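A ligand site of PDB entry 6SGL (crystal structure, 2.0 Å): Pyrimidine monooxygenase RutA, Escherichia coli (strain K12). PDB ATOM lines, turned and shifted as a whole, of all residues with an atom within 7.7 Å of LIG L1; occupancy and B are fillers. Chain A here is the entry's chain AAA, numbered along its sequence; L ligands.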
ATOM      1  N   PHE A   7       8.925 -21.554 -36.964  1.00  0.00           N
ATOM      2  CA  PHE A   7       7.905 -22.458 -36.465  1.00  0.00           C
ATOM      3  C   PHE A   7       6.706 -22.354 -37.410  1.00  0.00           C
ATOM      4  O   PHE A   7       6.012 -21.337 -37.405  1.00  0.00           O
ATOM      5  CB  PHE A   7       7.543 -22.039 -35.041  1.00  0.00           C
ATOM      6  CG  PHE A   7       7.092 -23.126 -34.095  1.00  0.00           C
ATOM      7  CD1 PHE A   7       7.282 -24.471 -34.388  1.00  0.00           C
ATOM      8  CD2 PHE A   7       6.482 -22.818 -32.904  1.00  0.00           C
ATOM      9  CE1 PHE A   7       6.869 -25.479 -33.513  1.00  0.00           C
ATOM     10  CE2 PHE A   7       6.107 -23.809 -32.005  1.00  0.00           C
ATOM     11  CZ  PHE A   7       6.282 -25.144 -32.309  1.00  0.00           C
ATOM     12  N   GLY A  14      -1.990 -19.839 -36.758  1.00  0.00           N
ATOM     13  CA  GLY A  14      -0.631 -19.797 -36.229  1.00  0.00           C
ATOM     14  C   GLY A  14      -0.673 -19.734 -34.706  1.00  0.00           C
ATOM     15  O   GLY A  14      -1.186 -20.652 -34.070  1.00  0.00           O
ATOM     16  N   TRP A  15      -0.064 -18.692 -34.113  1.00  0.00           N
ATOM     17  CA  TRP A  15       0.000 -18.713 -32.657  1.00  0.00           C
ATOM     18  C   TRP A  15      -0.794 -17.563 -32.015  1.00  0.00           C
ATOM     19  O   TRP A  15      -0.495 -17.195 -30.884  1.00  0.00           O
ATOM     20  CB  TRP A  15       1.440 -18.837 -32.125  1.00  0.00           C
ATOM     21  CG  TRP A  15       1.953 -20.250 -32.165  1.00  0.00           C
ATOM     22  CD1 TRP A  15       2.070 -21.134 -31.132  1.00  0.00           C
ATOM     23  CD2 TRP A  15       2.390 -20.937 -33.350  1.00  0.00           C
ATOM     24  NE1 TRP A  15       2.583 -22.328 -31.597  1.00  0.00           N
ATOM     25  CE2 TRP A  15       2.796 -22.234 -32.951  1.00  0.00           C
ATOM     26  CE3 TRP A  15       2.543 -20.565 -34.688  1.00  0.00           C
ATOM     27  CZ2 TRP A  15       3.275 -23.194 -33.855  1.00  0.00           C
ATOM     28  CZ3 TRP A  15       3.031 -21.497 -35.579  1.00  0.00           C
ATOM     29  CH2 TRP A  15       3.388 -22.788 -35.167  1.00  0.00           C
ATOM     30  N   MET A  49       5.261 -28.416 -35.323  1.00  0.00           N
ATOM     31  CA  MET A  49       4.664 -29.183 -34.245  1.00  0.00           C
ATOM     32  C   MET A  49       3.708 -30.261 -34.773  1.00  0.00           C
ATOM     33  O   MET A  49       3.520 -30.409 -35.978  1.00  0.00           O
ATOM     34  CB  MET A  49       3.924 -28.229 -33.305  1.00  0.00           C
ATOM     35  CG  MET A  49       2.776 -27.451 -33.972  1.00  0.00           C
ATOM     36  SD  MET A  49       1.705 -26.741 -32.653  1.00  0.00           S
ATOM     37  CE  MET A  49       0.356 -26.173 -33.688  1.00  0.00           C
ATOM     38  N   ILE A  50       3.154 -31.056 -33.855  1.00  0.00           N
ATOM     39  CA  ILE A  50       2.027 -31.929 -34.155  1.00  0.00           C
ATOM     40  C   ILE A  50       0.946 -31.588 -33.112  1.00  0.00           C
ATOM     41  O   ILE A  50       1.258 -31.367 -31.946  1.00  0.00           O
ATOM     42  CB  ILE A  50       2.428 -33.431 -34.171  1.00  0.00           C
ATOM     43  CG1 ILE A  50       1.292 -34.367 -34.614  1.00  0.00           C
ATOM     44  CG2 ILE A  50       2.989 -33.847 -32.808  1.00  0.00           C
ATOM     45  CD1 ILE A  50       0.842 -34.258 -36.089  1.00  0.00           C
ATOM     46  N   LYS A  51      -0.299 -31.439 -33.555  1.00  0.00           N
ATOM     47  CA  LYS A  51      -1.382 -31.072 -32.638  1.00  0.00           C
ATOM     48  C   LYS A  51      -2.698 -31.735 -33.063  1.00  0.00           C
ATOM     49  O   LYS A  51      -3.384 -31.269 -33.984  1.00  0.00           O
ATOM     50  CB  LYS A  51      -1.488 -29.552 -32.519  1.00  0.00           C
ATOM     51  CG  LYS A  51      -2.609 -29.005 -31.628  1.00  0.00           C
ATOM     52  CD  LYS A  51      -2.563 -29.330 -30.147  1.00  0.00           C
ATOM     53  CE  LYS A  51      -1.459 -28.593 -29.410  1.00  0.00           C
ATOM     54  NZ  LYS A  51      -0.192 -29.369 -29.470  1.00  0.00           N
ATOM     55  N   PHE A  55      -8.709 -26.147 -29.762  1.00  0.00           N
ATOM     56  CA  PHE A  55      -9.211 -25.468 -28.576  1.00  0.00           C
ATOM     57  C   PHE A  55     -10.570 -24.787 -28.769  1.00  0.00           C
ATOM     58  O   PHE A  55     -11.079 -24.202 -27.816  1.00  0.00           O
ATOM     59  CB  PHE A  55      -8.169 -24.472 -28.085  1.00  0.00           C
ATOM     60  CG  PHE A  55      -6.904 -25.169 -27.688  1.00  0.00           C
ATOM     61  CD1 PHE A  55      -6.936 -26.227 -26.791  1.00  0.00           C
ATOM     62  CD2 PHE A  55      -5.693 -24.798 -28.254  1.00  0.00           C
ATOM     63  CE1 PHE A  55      -5.777 -26.902 -26.442  1.00  0.00           C
ATOM     64  CE2 PHE A  55      -4.526 -25.469 -27.893  1.00  0.00           C
ATOM     65  CZ  PHE A  55      -4.571 -26.510 -27.000  1.00  0.00           C
ATOM     66  N   TRP A  62      -6.722 -24.063 -33.745  1.00  0.00           N
ATOM     67  CA  TRP A  62      -6.028 -25.344 -33.902  1.00  0.00           C
ATOM     68  C   TRP A  62      -6.979 -26.522 -34.055  1.00  0.00           C
ATOM     69  O   TRP A  62      -6.551 -27.684 -33.902  1.00  0.00           O
ATOM     70  CB  TRP A  62      -4.990 -25.612 -32.802  1.00  0.00           C
ATOM     71  CG  TRP A  62      -3.762 -24.760 -32.882  1.00  0.00           C
ATOM     72  CD1 TRP A  62      -3.426 -23.891 -33.882  1.00  0.00           C
ATOM     73  CD2 TRP A  62      -2.676 -24.745 -31.942  1.00  0.00           C
ATOM     74  NE1 TRP A  62      -2.217 -23.292 -33.603  1.00  0.00           N
ATOM     75  CE2 TRP A  62      -1.751 -23.780 -32.412  1.00  0.00           C
ATOM     76  CE3 TRP A  62      -2.445 -25.385 -30.715  1.00  0.00           C
ATOM     77  CZ2 TRP A  62      -0.570 -23.484 -31.715  1.00  0.00           C
ATOM     78  CZ3 TRP A  62      -1.273 -25.107 -30.042  1.00  0.00           C
ATOM     79  CH2 TRP A  62      -0.350 -24.172 -30.537  1.00  0.00           C
ATOM     80  N   VAL A 118       8.454 -35.732 -28.716  1.00  0.00           N
ATOM     81  CA  VAL A 118       7.648 -35.212 -27.620  1.00  0.00           C
ATOM     82  C   VAL A 118       6.921 -36.388 -26.963  1.00  0.00           C
ATOM     83  O   VAL A 118       6.541 -37.375 -27.615  1.00  0.00           O
ATOM     84  CB  VAL A 118       6.638 -34.136 -28.095  1.00  0.00           C
ATOM     85  CG1 VAL A 118       7.328 -32.912 -28.696  1.00  0.00           C
ATOM     86  CG2 VAL A 118       5.615 -34.720 -29.043  1.00  0.00           C
ATOM     87  N   TRP A 121       1.632 -33.916 -23.750  1.00  0.00           N
ATOM     88  CA  TRP A 121       1.129 -33.403 -22.490  1.00  0.00           C
ATOM     89  C   TRP A 121      -0.407 -33.494 -22.451  1.00  0.00           C
ATOM     90  O   TRP A 121      -0.976 -33.910 -21.441  1.00  0.00           O
ATOM     91  CB  TRP A 121       1.666 -31.989 -22.216  1.00  0.00           C
ATOM     92  CG  TRP A 121       1.215 -30.920 -23.169  1.00  0.00           C
ATOM     93  CD1 TRP A 121       1.853 -30.492 -24.295  1.00  0.00           C
ATOM     94  CD2 TRP A 121       0.006 -30.126 -23.074  1.00  0.00           C
ATOM     95  NE1 TRP A 121       1.138 -29.496 -24.911  1.00  0.00           N
ATOM     96  CE2 TRP A 121      -0.001 -29.251 -24.186  1.00  0.00           C
ATOM     97  CE3 TRP A 121      -1.061 -30.075 -22.168  1.00  0.00           C
ATOM     98  CZ2 TRP A 121      -1.027 -28.332 -24.405  1.00  0.00           C
ATOM     99  CZ3 TRP A 121      -2.081 -29.169 -22.388  1.00  0.00           C
ATOM    100  CH2 TRP A 121      -2.061 -28.312 -23.496  1.00  0.00           C
ATOM    101  N   GLN A 122      -1.043 -33.143 -23.584  1.00  0.00           N
ATOM    102  CA  GLN A 122      -2.477 -32.894 -23.685  1.00  0.00           C
ATOM    103  C   GLN A 122      -3.227 -34.222 -23.709  1.00  0.00           C
ATOM    104  O   GLN A 122      -3.397 -34.815 -24.785  1.00  0.00           O
ATOM    105  CB  GLN A 122      -2.775 -31.981 -24.891  1.00  0.00           C
ATOM    106  CG  GLN A 122      -4.232 -31.527 -25.034  1.00  0.00           C
ATOM    107  CD  GLN A 122      -4.437 -30.521 -26.143  1.00  0.00           C
ATOM    108  OE1 GLN A 122      -3.493 -29.923 -26.657  1.00  0.00           O
ATOM    109  NE2 GLN A 122      -5.677 -30.317 -26.541  1.00  0.00           N
ATOM    110  N   GLU A 125      -5.762 -35.186 -26.464  1.00  0.00           N
ATOM    111  CA  GLU A 125      -5.212 -35.506 -27.775  1.00  0.00           C
ATOM    112  C   GLU A 125      -5.130 -37.022 -27.992  1.00  0.00           C
ATOM    113  O   GLU A 125      -5.179 -37.462 -29.140  1.00  0.00           O
ATOM    114  CB  GLU A 125      -3.819 -34.912 -27.954  1.00  0.00           C
ATOM    115  CG  GLU A 125      -3.827 -33.628 -28.758  1.00  0.00           C
ATOM    116  CD  GLU A 125      -2.465 -32.972 -28.914  1.00  0.00           C
ATOM    117  OE1 GLU A 125      -1.810 -33.207 -29.961  1.00  0.00           O
ATOM    118  OE2 GLU A 125      -2.062 -32.201 -28.000  1.00  0.00           O
ATOM    119  N   PHE A 208      10.980 -22.136 -23.985  1.00  0.00           N
ATOM    120  CA  PHE A 208      10.142 -20.953 -24.167  1.00  0.00           C
ATOM    121  C   PHE A 208      10.913 -19.671 -23.868  1.00  0.00           C
ATOM    122  O   PHE A 208      11.587 -19.590 -22.855  1.00  0.00           O
ATOM    123  CB  PHE A 208       8.909 -21.055 -23.262  1.00  0.00           C
ATOM    124  CG  PHE A 208       8.017 -22.220 -23.595  1.00  0.00           C
ATOM    125  CD1 PHE A 208       7.192 -22.178 -24.711  1.00  0.00           C
ATOM    126  CD2 PHE A 208       8.052 -23.383 -22.847  1.00  0.00           C
ATOM    127  CE1 PHE A 208       6.397 -23.263 -25.042  1.00  0.00           C
ATOM    128  CE2 PHE A 208       7.250 -24.473 -23.171  1.00  0.00           C
ATOM    129  CZ  PHE A 208       6.413 -24.398 -24.262  1.00  0.00           C
ATOM    130  N   LEU A 241      11.959 -20.117 -28.143  1.00  0.00           N
ATOM    131  CA  LEU A 241      10.786 -19.766 -28.950  1.00  0.00           C
ATOM    132  C   LEU A 241      10.291 -18.346 -28.620  1.00  0.00           C
ATOM    133  O   LEU A 241       9.953 -18.082 -27.468  1.00  0.00           O
ATOM    134  CB  LEU A 241       9.703 -20.787 -28.648  1.00  0.00           C
ATOM    135  CG  LEU A 241       8.307 -20.413 -29.175  1.00  0.00           C
ATOM    136  CD1 LEU A 241       8.303 -20.300 -30.702  1.00  0.00           C
ATOM    137  CD2 LEU A 241       7.312 -21.466 -28.734  1.00  0.00           C
ATOM    138  N   LEU A 272      -7.728 -23.827 -22.884  1.00  0.00           N
ATOM    139  CA  LEU A 272      -6.297 -23.954 -22.647  1.00  0.00           C
ATOM    140  C   LEU A 272      -6.036 -24.244 -21.169  1.00  0.00           C
ATOM    141  O   LEU A 272      -5.117 -25.003 -20.849  1.00  0.00           O
ATOM    142  CB  LEU A 272      -5.585 -22.668 -23.105  1.00  0.00           C
ATOM    143  CG  LEU A 272      -4.412 -22.828 -24.062  1.00  0.00           C
ATOM    144  CD1 LEU A 272      -3.543 -24.049 -23.728  1.00  0.00           C
ATOM    145  CD2 LEU A 272      -4.894 -22.903 -25.514  1.00  0.00           C
ATOM    146  N   ASN A 299      -1.268 -15.372 -27.240  1.00  0.00           N
ATOM    147  CA  ASN A 299      -0.301 -16.247 -27.890  1.00  0.00           C
ATOM    148  C   ASN A 299       0.252 -17.282 -26.926  1.00  0.00           C
ATOM    149  O   ASN A 299       1.441 -17.604 -27.009  1.00  0.00           O
ATOM    150  CB  ASN A 299       0.840 -15.474 -28.559  1.00  0.00           C
ATOM    151  CG  ASN A 299       1.646 -14.644 -27.587  1.00  0.00           C
ATOM    152  OD1 ASN A 299       1.504 -14.786 -26.372  1.00  0.00           O
ATOM    153  ND2 ASN A 299       2.472 -13.762 -28.118  1.00  0.00           N
ATOM    154  N   ILE A 300      -0.610 -17.785 -26.031  1.00  0.00           N
ATOM    155  CA  ILE A 300      -0.277 -18.828 -25.050  1.00  0.00           C
ATOM    156  C   ILE A 300       0.852 -18.348 -24.129  1.00  0.00           C
ATOM    157  O   ILE A 300       1.716 -19.119 -23.710  1.00  0.00           O
ATOM    158  CB  ILE A 300       0.006 -20.198 -25.718  1.00  0.00           C
ATOM    159  CG1 ILE A 300      -1.055 -20.546 -26.775  1.00  0.00           C
ATOM    160  CG2 ILE A 300       0.116 -21.308 -24.678  1.00  0.00           C
ATOM    161  CD1 ILE A 300      -0.539 -21.336 -27.969  1.00  0.00           C
ATOM    162  N   MET A 302       3.367 -16.548 -24.869  1.00  0.00           N
ATOM    163  CA  MET A 302       4.666 -16.787 -25.476  1.00  0.00           C
ATOM    164  C   MET A 302       5.593 -15.630 -25.121  1.00  0.00           C
ATOM    165  O   MET A 302       5.154 -14.506 -24.895  1.00  0.00           O
ATOM    166  CB  MET A 302       4.486 -16.864 -27.006  1.00  0.00           C
ATOM    167  CG  MET A 302       5.648 -17.542 -27.711  1.00  0.00           C
ATOM    168  SD  MET A 302       5.345 -17.786 -29.481  1.00  0.00           S
ATOM    169  CE  MET A 302       4.084 -19.052 -29.384  1.00  0.00           C
ATOM    170  N   THR A 331       7.930 -17.475 -34.338  1.00  0.00           N
ATOM    171  CA  THR A 331       6.645 -17.204 -34.956  1.00  0.00           C
ATOM    172  C   THR A 331       6.491 -15.698 -35.225  1.00  0.00           C
ATOM    173  O   THR A 331       7.242 -14.841 -34.708  1.00  0.00           O
ATOM    174  CB  THR A 331       5.515 -17.691 -34.053  1.00  0.00           C
ATOM    175  OG1 THR A 331       5.665 -16.911 -32.871  1.00  0.00           O
ATOM    176  CG2 THR A 331       5.610 -19.161 -33.710  1.00  0.00           C
HETATM  177  N1  LIG L   1       3.254 -24.327 -28.494  1.00  0.00           N
HETATM  178  C1  LIG L   1       2.933 -24.752 -27.231  1.00  0.00           C
HETATM  179  O1  LIG L   1       3.071 -24.057 -26.228  1.00  0.00           O
HETATM  180  N2  LIG L   1       2.442 -26.047 -27.150  1.00  0.00           N
HETATM  181  C2  LIG L   1       2.256 -26.919 -28.216  1.00  0.00           C
HETATM  182  O2  LIG L   1       1.795 -28.035 -28.007  1.00  0.00           O
HETATM  183  C3  LIG L   1       2.619 -26.376 -29.500  1.00  0.00           C
HETATM  184  C4  LIG L   1       3.099 -25.116 -29.601  1.00  0.00           C
HETATM  185  N1  LG2 L   2       4.136 -30.655 -27.407  1.00  0.00           N
HETATM  186  C1  LG2 L   2       3.394 -31.460 -28.210  1.00  0.00           C
HETATM  187  O1  LG2 L   2       2.574 -32.243 -27.690  1.00  0.00           O
HETATM  188  N2  LG2 L   2       3.516 -31.450 -29.562  1.00  0.00           N
HETATM  189  C2  LG2 L   2       4.387 -30.610 -30.172  1.00  0.00           C
HETATM  190  O2  LG2 L   2       4.503 -30.645 -31.405  1.00  0.00           O
HETATM  191  C3  LG2 L   2       5.270 -29.695 -29.376  1.00  0.00           C
HETATM  192  N3  LG2 L   2       6.186 -28.848 -29.906  1.00  0.00           N
HETATM  193  C4  LG2 L   2       6.915 -28.016 -29.118  1.00  0.00           C
HETATM  194  C5  LG2 L   2       7.853 -27.130 -29.697  1.00  0.00           C
HETATM  195  C6  LG2 L   2       8.592 -26.253 -28.918  1.00  0.00           C
HETATM  196  C7  LG2 L   2       9.555 -25.360 -29.619  1.00  0.00           C
HETATM  197  C8  LG2 L   2       8.432 -26.264 -27.403  1.00  0.00           C
HETATM  198  C9  LG2 L   2       9.225 -25.389 -26.468  1.00  0.00           C
HETATM  199  C10 LG2 L   2       7.502 -27.130 -26.816  1.00  0.00           C
HETATM  200  C11 LG2 L   2       6.742 -28.008 -27.624  1.00  0.00           C
HETATM  201  N4  LG2 L   2       5.809 -28.915 -27.052  1.00  0.00           N
HETATM  202  C12 LG2 L   2       5.069 -29.770 -27.905  1.00  0.00           C
HETATM  203  C13 LG2 L   2       5.563 -29.017 -25.605  1.00  0.00           C
HETATM  204  C14 LG2 L   2       6.848 -29.437 -24.916  1.00  0.00           C
HETATM  205  O3  LG2 L   2       7.098 -30.821 -25.232  1.00  0.00           O
HETATM  206  C15 LG2 L   2       6.781 -28.964 -23.433  1.00  0.00           C
HETATM  207  O4  LG2 L   2       7.795 -27.999 -23.105  1.00  0.00           O
HETATM  208  C16 LG2 L   2       6.938 -30.092 -22.471  1.00  0.00           C
HETATM  209  O5  LG2 L   2       5.899 -31.043 -22.733  1.00  0.00           O
HETATM  210  C17 LG2 L   2       7.024 -29.548 -21.026  1.00  0.00           C
HETATM  211  O6  LG2 L   2       8.305 -30.038 -20.551  1.00  0.00           O
HETATM  212  P1  LG2 L   2       8.367 -31.504 -19.894  1.00  0.00           P
HETATM  213  O7  LG2 L   2       7.890 -32.498 -20.939  1.00  0.00           O
HETATM  214  O8  LG2 L   2       9.825 -31.704 -19.571  1.00  0.00           O
HETATM  215  O9  LG2 L   2       7.413 -31.330 -18.757  1.00  0.00           O
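OE2 of Glu 125 lies within salt-bridge range of NZ of Lys 51, 3.7 Å away.
NE1 of Trp 62 sits at hydrogen-bond distance from O of Gly 14 (2.9 Å).
NZ of Lys 51 is in hydrogen-bond range of O2 of LIG L1, at 2.8 Å.
O of Ile 50 lies within hydrogen-bond range of N2 of LG2 L2 (3.3 Å).
An oxygen (O2) of LIG L1 sits at hydrogen-bond distance from the indole nitrogen (NE1) of Trp 121 (3.5 Å).
N of Ile 50 is in hydrogen-bond range of O2 of LG2 L2.
NE1 of Trp 15 touches C4 of LIG L1 (3.5 Å).
Met 49 touches LIG L1.
Trp 62 touches LIG L1 (CH2 to C4, 3.7 Å).
CE1 of Phe 208 touches O1 of LIG L1, at 3.6 Å.
Within 4 Å of LIG L1: Trp 15, Met 49, Lys 51, Trp 62, Trp 121 and Phe 208.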
